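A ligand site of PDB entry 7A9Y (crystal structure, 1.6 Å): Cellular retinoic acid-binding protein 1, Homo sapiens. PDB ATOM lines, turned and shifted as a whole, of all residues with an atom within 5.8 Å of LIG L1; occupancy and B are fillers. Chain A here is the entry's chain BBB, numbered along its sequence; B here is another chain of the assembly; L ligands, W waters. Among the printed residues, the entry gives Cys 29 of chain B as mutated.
An oxygen (O1) of LIG L1 is in hydrogen-bond range of the side-chain hydroxyl (OH) of Tyr 134, 2.7 Å away. An oxygen (O1) of LIG L1 is in salt-bridge range of the guanidinium group (NE) of Arg 132, at 2.8 Å.
NH1 of Arg 60 lies within hydrogen-bond range of O of Val 77 (3.0 Å). O of Pro 40 lies within hydrogen-bond range of N of Met 10 (3.4 Å). The guanidinium group (NH2) of Arg 132 lies close to the side-chain sulfur (SD) of Met 10 (3.5 Å). The backbone NH of Arg 132 lies within hydrogen-bond range of the backbone carbonyl oxygen of Leu 121 (2.8 Å). NH2 of Arg 132 is in hydrogen-bond range of O of Ala 37 (2.8 Å). OG1 of Thr 57 lies within hydrogen-bond range of O of Arg 60 (2.8 Å).
CG1 of Val 32 of chain A touches C13 of LIG L1, at 3.4 Å. Ala 33 of chain A touches LIG L1 (CA to C9, 3.9 Å). CB of Ala 37 touches C5 of LIG L1, at 3.6 Å. CG of Pro 40 touches O1 of LIG L1 (3.95 Å). Thr 55 touches LIG L1 (CG2 to O2, 3.6 Å). NE of Arg 60 touches C8 of LIG L1, 3.8 Å away. Leu 121 touches LIG L1. Phe 123 touches LIG L1 (CE2 to C2, 3.8 Å). SG of Cys 29 of chain B touches C12 of LIG L1, 3.7 Å away. Val 32 of chain B touches LIG L1 (CG1 to C13, 3.8 Å). CG1 of Val 59 of chain B touches C14 of LIG L1, at 3.7 Å. Hydrophobic or aromatic side chains that line LIG L1: Val 32 of chain A, Ala 33 of chain A, Ala 37, Pro 40, Leu 121, Phe 123, Tyr 134, Val 32 of chain B and Val 59 of chain B. Within 4 Å of LIG L1: Val 32 of chain A, Ala 33 of chain A, Ala 37, Pro 40, Thr 55, Arg 60, Leu 121, Phe 123, Arg 132, Tyr 134, Cys 29 of chain B, Val 32 of chain B and Val 59 of chain B. The nearest printed residue that does not touch LIG L1 is Met 28 of chain B (4.1 Å).
Water W1 lies within hydrogen-bond range of an oxygen (O2) of LIG L1 (2.7 Å), the side-chain hydroxyl (OG1) of Thr 55 (2.9 Å) and the guanidinium group (NH2) of Arg 112 (2.9 Å).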
ATOM      1  N   MET A  10       8.478  -5.689  31.936  1.00  0.00           N
ATOM      2  CA  MET A  10       9.267  -4.925  30.922  1.00  0.00           C
ATOM      3  C   MET A  10       9.570  -3.546  31.479  1.00  0.00           C
ATOM      4  O   MET A  10       8.639  -2.936  32.036  1.00  0.00           O
ATOM      5  CB  MET A  10       8.544  -4.790  29.591  1.00  0.00           C
ATOM      6  CG  MET A  10       9.503  -4.350  28.525  1.00  0.00           C
ATOM      7  SD  MET A  10       8.739  -4.388  26.924  1.00  0.00           S
ATOM      8  CE  MET A  10       7.763  -2.899  27.102  1.00  0.00           C
ATOM      9  N   PHE A  16      10.123  -0.484  18.589  1.00  0.00           N
ATOM     10  CA  PHE A  16       8.973  -1.383  18.342  1.00  0.00           C
ATOM     11  C   PHE A  16       8.109  -0.852  17.194  1.00  0.00           C
ATOM     12  O   PHE A  16       7.656  -1.664  16.336  1.00  0.00           O
ATOM     13  CB  PHE A  16       8.156  -1.615  19.598  1.00  0.00           C
ATOM     14  CG  PHE A  16       7.140  -2.730  19.513  1.00  0.00           C
ATOM     15  CD1 PHE A  16       7.496  -3.984  19.078  1.00  0.00           C
ATOM     16  CD2 PHE A  16       5.811  -2.516  19.824  1.00  0.00           C
ATOM     17  CE1 PHE A  16       6.574  -5.027  19.055  1.00  0.00           C
ATOM     18  CE2 PHE A  16       4.877  -3.532  19.771  1.00  0.00           C
ATOM     19  CZ  PHE A  16       5.254  -4.785  19.367  1.00  0.00           C
ATOM     20  N   VAL A  32      -1.935   1.583  18.241  1.00  0.00           N
ATOM     21  CA  VAL A  32      -2.702   0.752  19.219  1.00  0.00           C
ATOM     22  C   VAL A  32      -1.800  -0.391  19.693  1.00  0.00           C
ATOM     23  O   VAL A  32      -1.806  -0.732  20.908  1.00  0.00           O
ATOM     24  CB  VAL A  32      -3.986   0.237  18.554  1.00  0.00           C
ATOM     25  CG1 VAL A  32      -4.687  -0.829  19.377  1.00  0.00           C
ATOM     26  CG2 VAL A  32      -4.935   1.390  18.256  1.00  0.00           C
ATOM     27  N   ALA A  33      -1.096  -1.032  18.793  1.00  0.00           N
ATOM     28  CA  ALA A  33      -0.278  -2.203  19.165  1.00  0.00           C
ATOM     29  C   ALA A  33       0.881  -1.780  20.080  1.00  0.00           C
ATOM     30  O   ALA A  33       1.201  -2.544  21.040  1.00  0.00           O
ATOM     31  CB  ALA A  33       0.244  -2.869  17.923  1.00  0.00           C
ATOM     32  N   ALA A  36      -0.712  -1.244  23.493  1.00  0.00           N
ATOM     33  CA  ALA A  36      -1.160  -2.526  24.070  1.00  0.00           C
ATOM     34  C   ALA A  36       0.018  -3.376  24.584  1.00  0.00           C
ATOM     35  O   ALA A  36      -0.178  -4.125  25.545  1.00  0.00           O
ATOM     36  CB  ALA A  36      -1.946  -3.299  23.014  1.00  0.00           C
ATOM     37  N   ALA A  37       1.206  -3.246  23.967  1.00  0.00           N
ATOM     38  CA  ALA A  37       2.417  -4.033  24.253  1.00  0.00           C
ATOM     39  C   ALA A  37       3.377  -3.259  25.179  1.00  0.00           C
ATOM     40  O   ALA A  37       4.482  -3.731  25.356  1.00  0.00           O
ATOM     41  CB  ALA A  37       3.133  -4.387  22.974  1.00  0.00           C
ATOM     42  N   PRO A  40       4.217  -5.733  29.069  1.00  0.00           N
ATOM     43  CA  PRO A  40       3.936  -7.140  29.253  1.00  0.00           C
ATOM     44  C   PRO A  40       4.556  -7.690  30.549  1.00  0.00           C
ATOM     45  O   PRO A  40       5.613  -7.234  31.010  1.00  0.00           O
ATOM     46  CB  PRO A  40       4.550  -7.785  27.994  1.00  0.00           C
ATOM     47  CG  PRO A  40       4.886  -6.667  27.056  1.00  0.00           C
ATOM     48  CD  PRO A  40       5.096  -5.438  27.930  1.00  0.00           C
ATOM     49  N   VAL A  42       5.878 -11.430  31.869  1.00  0.00           N
ATOM     50  CA  VAL A  42       6.404 -12.684  31.287  1.00  0.00           C
ATOM     51  C   VAL A  42       6.658 -13.688  32.404  1.00  0.00           C
ATOM     52  O   VAL A  42       7.231 -13.288  33.442  1.00  0.00           O
ATOM     53  CB  VAL A  42       7.665 -12.363  30.467  1.00  0.00           C
ATOM     54  CG1 VAL A  42       8.441 -13.618  30.123  1.00  0.00           C
ATOM     55  CG2 VAL A  42       7.265 -11.593  29.222  1.00  0.00           C
ATOM     56  N   THR A  55       3.817 -14.748  27.650  1.00  0.00           N
ATOM     57  CA  THR A  55       3.840 -13.280  27.588  1.00  0.00           C
ATOM     58  C   THR A  55       2.420 -12.785  27.651  1.00  0.00           C
ATOM     59  O   THR A  55       1.624 -13.116  26.756  1.00  0.00           O
ATOM     60  CB  THR A  55       4.581 -12.787  26.344  1.00  0.00           C
ATOM     61  OG1 THR A  55       5.886 -13.353  26.319  1.00  0.00           O
ATOM     62  CG2 THR A  55       4.716 -11.284  26.312  1.00  0.00           C
ATOM     63  N   THR A  57      -0.420  -9.637  28.134  1.00  0.00           N
ATOM     64  CA  THR A  57      -0.947  -8.259  28.155  1.00  0.00           C
ATOM     65  C   THR A  57      -2.440  -8.390  28.333  1.00  0.00           C
ATOM     66  O   THR A  57      -2.956  -9.477  28.127  1.00  0.00           O
ATOM     67  CB  THR A  57      -0.552  -7.498  26.884  1.00  0.00           C
ATOM     68  OG1 THR A  57      -1.271  -8.058  25.779  1.00  0.00           O
ATOM     69  CG2 THR A  57       0.933  -7.576  26.562  1.00  0.00           C
ATOM     70  N   VAL A  59      -4.683  -7.349  26.374  1.00  0.00           N
ATOM     71  CA  VAL A  59      -5.375  -7.607  25.081  1.00  0.00           C
ATOM     72  C   VAL A  59      -4.942  -8.951  24.480  1.00  0.00           C
ATOM     73  O   VAL A  59      -5.729  -9.452  23.661  1.00  0.00           O
ATOM     74  CB  VAL A  59      -5.241  -6.470  24.047  1.00  0.00           C
ATOM     75  CG1 VAL A  59      -5.698  -5.153  24.651  1.00  0.00           C
ATOM     76  CG2 VAL A  59      -3.852  -6.341  23.484  1.00  0.00           C
ATOM     77  N   ARG A  60      -3.770  -9.483  24.782  1.00  0.00           N
ATOM     78  CA  ARG A  60      -3.265 -10.695  24.094  1.00  0.00           C
ATOM     79  C   ARG A  60      -2.229 -11.438  24.931  1.00  0.00           C
ATOM     80  O   ARG A  60      -1.258 -10.839  25.468  1.00  0.00           O
ATOM     81  CB  ARG A  60      -2.709 -10.324  22.724  1.00  0.00           C
ATOM     82  CG  ARG A  60      -2.284 -11.513  21.869  1.00  0.00           C
ATOM     83  CD  ARG A  60      -1.678 -11.072  20.529  1.00  0.00           C
ATOM     84  NE  ARG A  60      -0.222 -10.984  20.589  1.00  0.00           N
ATOM     85  CZ  ARG A  60       0.595 -10.715  19.568  1.00  0.00           C
ATOM     86  NH1 ARG A  60       0.127 -10.410  18.367  1.00  0.00           N
ATOM     87  NH2 ARG A  60       1.901 -10.719  19.771  1.00  0.00           N
ATOM     88  N   VAL A  77       5.625 -11.684  15.785  1.00  0.00           N
ATOM     89  CA  VAL A  77       5.030 -10.622  16.647  1.00  0.00           C
ATOM     90  C   VAL A  77       3.672 -10.191  16.086  1.00  0.00           C
ATOM     91  O   VAL A  77       2.740  -9.926  16.871  1.00  0.00           O
ATOM     92  CB  VAL A  77       6.004  -9.416  16.706  1.00  0.00           C
ATOM     93  CG1 VAL A  77       5.388  -8.274  17.478  1.00  0.00           C
ATOM     94  CG2 VAL A  77       7.333  -9.807  17.287  1.00  0.00           C
ATOM     95  N   ARG A 112      16.934 -14.007  23.083  1.00  0.00           N
ATOM     96  CA  ARG A 112      16.732 -13.731  24.539  1.00  0.00           C
ATOM     97  C   ARG A 112      18.081 -13.959  25.205  1.00  0.00           C
ATOM     98  O   ARG A 112      18.655 -15.051  25.022  1.00  0.00           O
ATOM     99  CB  ARG A 112      15.607 -14.551  25.160  1.00  0.00           C
ATOM    100  CG  ARG A 112      14.195 -14.054  24.875  1.00  0.00           C
ATOM    101  CD  ARG A 112      13.145 -14.903  25.517  1.00  0.00           C
ATOM    102  NE  ARG A 112      11.816 -14.303  25.396  1.00  0.00           N
ATOM    103  CZ  ARG A 112      10.972 -14.559  24.424  1.00  0.00           C
ATOM    104  NH1 ARG A 112      11.287 -15.437  23.472  1.00  0.00           N
ATOM    105  NH2 ARG A 112       9.800 -13.938  24.437  1.00  0.00           N
ATOM    106  N   LEU A 121      15.365  -8.994  25.328  1.00  0.00           N
ATOM    107  CA  LEU A 121      14.636  -9.621  24.207  1.00  0.00           C
ATOM    108  C   LEU A 121      14.910  -8.754  22.969  1.00  0.00           C
ATOM    109  O   LEU A 121      14.673  -7.554  23.023  1.00  0.00           O
ATOM    110  CB  LEU A 121      13.143  -9.664  24.539  1.00  0.00           C
ATOM    111  CG  LEU A 121      12.221  -9.979  23.346  1.00  0.00           C
ATOM    112  CD1 LEU A 121      12.441 -11.413  22.867  1.00  0.00           C
ATOM    113  CD2 LEU A 121      10.780  -9.761  23.802  1.00  0.00           C
ATOM    114  N   PHE A 123      13.986  -8.449  18.765  1.00  0.00           N
ATOM    115  CA  PHE A 123      13.228  -8.898  17.578  1.00  0.00           C
ATOM    116  C   PHE A 123      13.864  -8.284  16.368  1.00  0.00           C
ATOM    117  O   PHE A 123      14.177  -7.074  16.369  1.00  0.00           O
ATOM    118  CB  PHE A 123      11.791  -8.403  17.627  1.00  0.00           C
ATOM    119  CG  PHE A 123      10.942  -9.018  18.704  1.00  0.00           C
ATOM    120  CD1 PHE A 123      10.696 -10.385  18.710  1.00  0.00           C
ATOM    121  CD2 PHE A 123      10.278  -8.226  19.625  1.00  0.00           C
ATOM    122  CE1 PHE A 123       9.863 -10.956  19.649  1.00  0.00           C
ATOM    123  CE2 PHE A 123       9.418  -8.800  20.547  1.00  0.00           C
ATOM    124  CZ  PHE A 123       9.239 -10.161  20.585  1.00  0.00           C
ATOM    125  N   ARG A 132      13.849  -5.026  23.835  1.00  0.00           N
ATOM    126  CA  ARG A 132      12.971  -4.916  25.010  1.00  0.00           C
ATOM    127  C   ARG A 132      13.701  -5.465  26.214  1.00  0.00           C
ATOM    128  O   ARG A 132      14.134  -6.612  26.170  1.00  0.00           O
ATOM    129  CB  ARG A 132      11.671  -5.593  24.687  1.00  0.00           C
ATOM    130  CG  ARG A 132      10.869  -4.683  23.789  1.00  0.00           C
ATOM    131  CD  ARG A 132       9.885  -5.335  22.873  1.00  0.00           C
ATOM    132  NE  ARG A 132       8.628  -5.617  23.535  1.00  0.00           N
ATOM    133  CZ  ARG A 132       7.598  -4.779  23.701  1.00  0.00           C
ATOM    134  NH1 ARG A 132       7.556  -3.552  23.225  1.00  0.00           N
ATOM    135  NH2 ARG A 132       6.533  -5.257  24.290  1.00  0.00           N
ATOM    136  N   TYR A 134      13.640  -6.536  30.170  1.00  0.00           N
ATOM    137  CA  TYR A 134      12.813  -7.072  31.278  1.00  0.00           C
ATOM    138  C   TYR A 134      13.695  -7.200  32.535  1.00  0.00           C
ATOM    139  O   TYR A 134      14.903  -7.505  32.462  1.00  0.00           O
ATOM    140  CB  TYR A 134      12.254  -8.413  30.863  1.00  0.00           C
ATOM    141  CG  TYR A 134      11.124  -8.372  29.860  1.00  0.00           C
ATOM    142  CD1 TYR A 134      11.347  -8.314  28.495  1.00  0.00           C
ATOM    143  CD2 TYR A 134       9.817  -8.449  30.287  1.00  0.00           C
ATOM    144  CE1 TYR A 134      10.288  -8.315  27.592  1.00  0.00           C
ATOM    145  CE2 TYR A 134       8.752  -8.447  29.421  1.00  0.00           C
ATOM    146  CZ  TYR A 134       8.989  -8.397  28.059  1.00  0.00           C
ATOM    147  OH  TYR A 134       7.884  -8.377  27.266  1.00  0.00           O
ATOM    148  N   MET B  28      -2.959  -8.121  12.476  1.00  0.00           N
ATOM    149  CA  MET B  28      -2.467  -8.181  13.880  1.00  0.00           C
ATOM    150  C   MET B  28      -3.534  -7.594  14.804  1.00  0.00           C
ATOM    151  O   MET B  28      -3.840  -8.197  15.894  1.00  0.00           O
ATOM    152  CB  MET B  28      -1.159  -7.366  13.959  1.00  0.00           C
ATOM    153  CG  MET B  28      -0.533  -7.408  15.336  1.00  0.00           C
ATOM    154  SD  MET B  28       0.955  -6.299  15.293  1.00  0.00           S
ATOM    155  CE  MET B  28       1.524  -6.491  16.986  1.00  0.00           C
ATOM    156  N   CYS B  29      -4.090  -6.455  14.379  1.00  0.00           N
ATOM    157  CA  CYS B  29      -5.171  -5.717  15.093  1.00  0.00           C
ATOM    158  C   CYS B  29      -6.532  -6.404  14.893  1.00  0.00           C
ATOM    159  O   CYS B  29      -7.276  -6.543  15.857  1.00  0.00           O
ATOM    160  CB  CYS B  29      -5.222  -4.268  14.622  1.00  0.00           C
ATOM    161  SG  CYS B  29      -3.859  -3.328  15.369  1.00  0.00           S
ATOM    162  N   VAL B  32      -7.177  -9.440  17.294  1.00  0.00           N
ATOM    163  CA  VAL B  32      -7.557  -9.049  18.688  1.00  0.00           C
ATOM    164  C   VAL B  32      -8.958  -8.472  18.675  1.00  0.00           C
ATOM    165  O   VAL B  32      -9.760  -8.831  19.568  1.00  0.00           O
ATOM    166  CB  VAL B  32      -6.525  -8.046  19.236  1.00  0.00           C
ATOM    167  CG1 VAL B  32      -6.952  -7.520  20.595  1.00  0.00           C
ATOM    168  CG2 VAL B  32      -5.164  -8.682  19.292  1.00  0.00           C
ATOM    169  N   ALA B  33      -9.239  -7.573  17.732  1.00  0.00           N
ATOM    170  CA  ALA B  33     -10.555  -6.860  17.654  1.00  0.00           C
ATOM    171  C   ALA B  33     -11.697  -7.853  17.512  1.00  0.00           C
ATOM    172  O   ALA B  33     -12.759  -7.674  18.143  1.00  0.00           O
ATOM    173  CB  ALA B  33     -10.561  -5.895  16.522  1.00  0.00           C
ATOM    174  N   VAL B  59     -10.662  -4.119  25.245  1.00  0.00           N
ATOM    175  CA  VAL B  59      -9.650  -3.573  24.301  1.00  0.00           C
ATOM    176  C   VAL B  59      -9.915  -2.100  24.027  1.00  0.00           C
ATOM    177  O   VAL B  59      -8.962  -1.344  23.760  1.00  0.00           O
ATOM    178  CB  VAL B  59      -9.632  -4.388  22.987  1.00  0.00           C
ATOM    179  CG1 VAL B  59      -8.863  -3.692  21.876  1.00  0.00           C
ATOM    180  CG2 VAL B  59      -9.086  -5.782  23.212  1.00  0.00           C
HETATM  181  C1  LIG L   1       7.180  -8.924  23.880  1.00  0.00           C
HETATM  182  O1  LIG L   1       7.703  -8.004  24.624  1.00  0.00           O
HETATM  183  O2  LIG L   1       7.296 -10.144  24.069  1.00  0.00           O
HETATM  184  C2  LIG L   1       6.283  -8.494  22.723  1.00  0.00           C
HETATM  185  C3  LIG L   1       4.820  -8.394  23.133  1.00  0.00           C
HETATM  186  C4  LIG L   1       3.920  -7.873  22.024  1.00  0.00           C
HETATM  187  C5  LIG L   1       2.451  -7.897  22.361  1.00  0.00           C
HETATM  188  C6  LIG L   1       1.541  -7.229  21.339  1.00  0.00           C
HETATM  189  C7  LIG L   1       0.086  -7.156  21.761  1.00  0.00           C
HETATM  190  C8  LIG L   1      -0.891  -7.202  20.604  1.00  0.00           C
HETATM  191  C9  LIG L   1      -1.170  -5.884  19.952  1.00  0.00           C
HETATM  192  C10 LIG L   1      -2.427  -5.830  19.091  1.00  0.00           C
HETATM  193  C11 LIG L   1      -3.513  -4.981  19.674  1.00  0.00           C
HETATM  194  C12 LIG L   1      -4.642  -4.654  18.752  1.00  0.00           C
HETATM  195  C13 LIG L   1      -5.821  -4.050  19.505  1.00  0.00           C
HETATM  196  C14 LIG L   1      -7.076  -3.779  18.688  1.00  0.00           C
HETATM  197  O1  LG2 L   2     -20.313  -3.329  18.121  1.00  0.00           O
HETATM  198  O2  LG2 L   2     -20.142  -1.205  18.447  1.00  0.00           O
HETATM  199  C1  LG2 L   2     -19.656  -2.324  18.114  1.00  0.00           C
HETATM  200  C2  LG2 L   2     -18.207  -2.393  17.729  1.00  0.00           C
HETATM  201  C3  LG2 L   2     -17.277  -2.379  18.918  1.00  0.00           C
HETATM  202  C4  LG2 L   2     -15.814  -2.205  18.495  1.00  0.00           C
HETATM  203  C5  LG2 L   2     -14.799  -2.614  19.521  1.00  0.00           C
HETATM  204  C6  LG2 L   2     -13.397  -2.902  18.984  1.00  0.00           C
HETATM  205  C7  LG2 L   2     -12.969  -2.058  17.794  1.00  0.00           C
HETATM  206  C8  LG2 L   2     -11.517  -2.189  17.413  1.00  0.00           C
HETATM  207  C9  LG2 L   2     -11.140  -1.460  16.136  1.00  0.00           C
HETATM  208  C10 LG2 L   2      -9.823  -1.886  15.504  1.00  0.00           C
HETATM  209  C11 LG2 L   2      -9.005  -0.766  14.922  1.00  0.00           C
HETATM  210  C12 LG2 L   2      -7.569  -0.725  15.353  1.00  0.00           C
HETATM  211  C13 LG2 L   2      -6.729   0.287  14.589  1.00  0.00           C
HETATM  212  O   HOH W   1       8.348 -11.873  25.900  1.00  0.00           O
HETATM  213  O   HOH W   2       6.009 -12.033  22.533  1.00  0.00           O
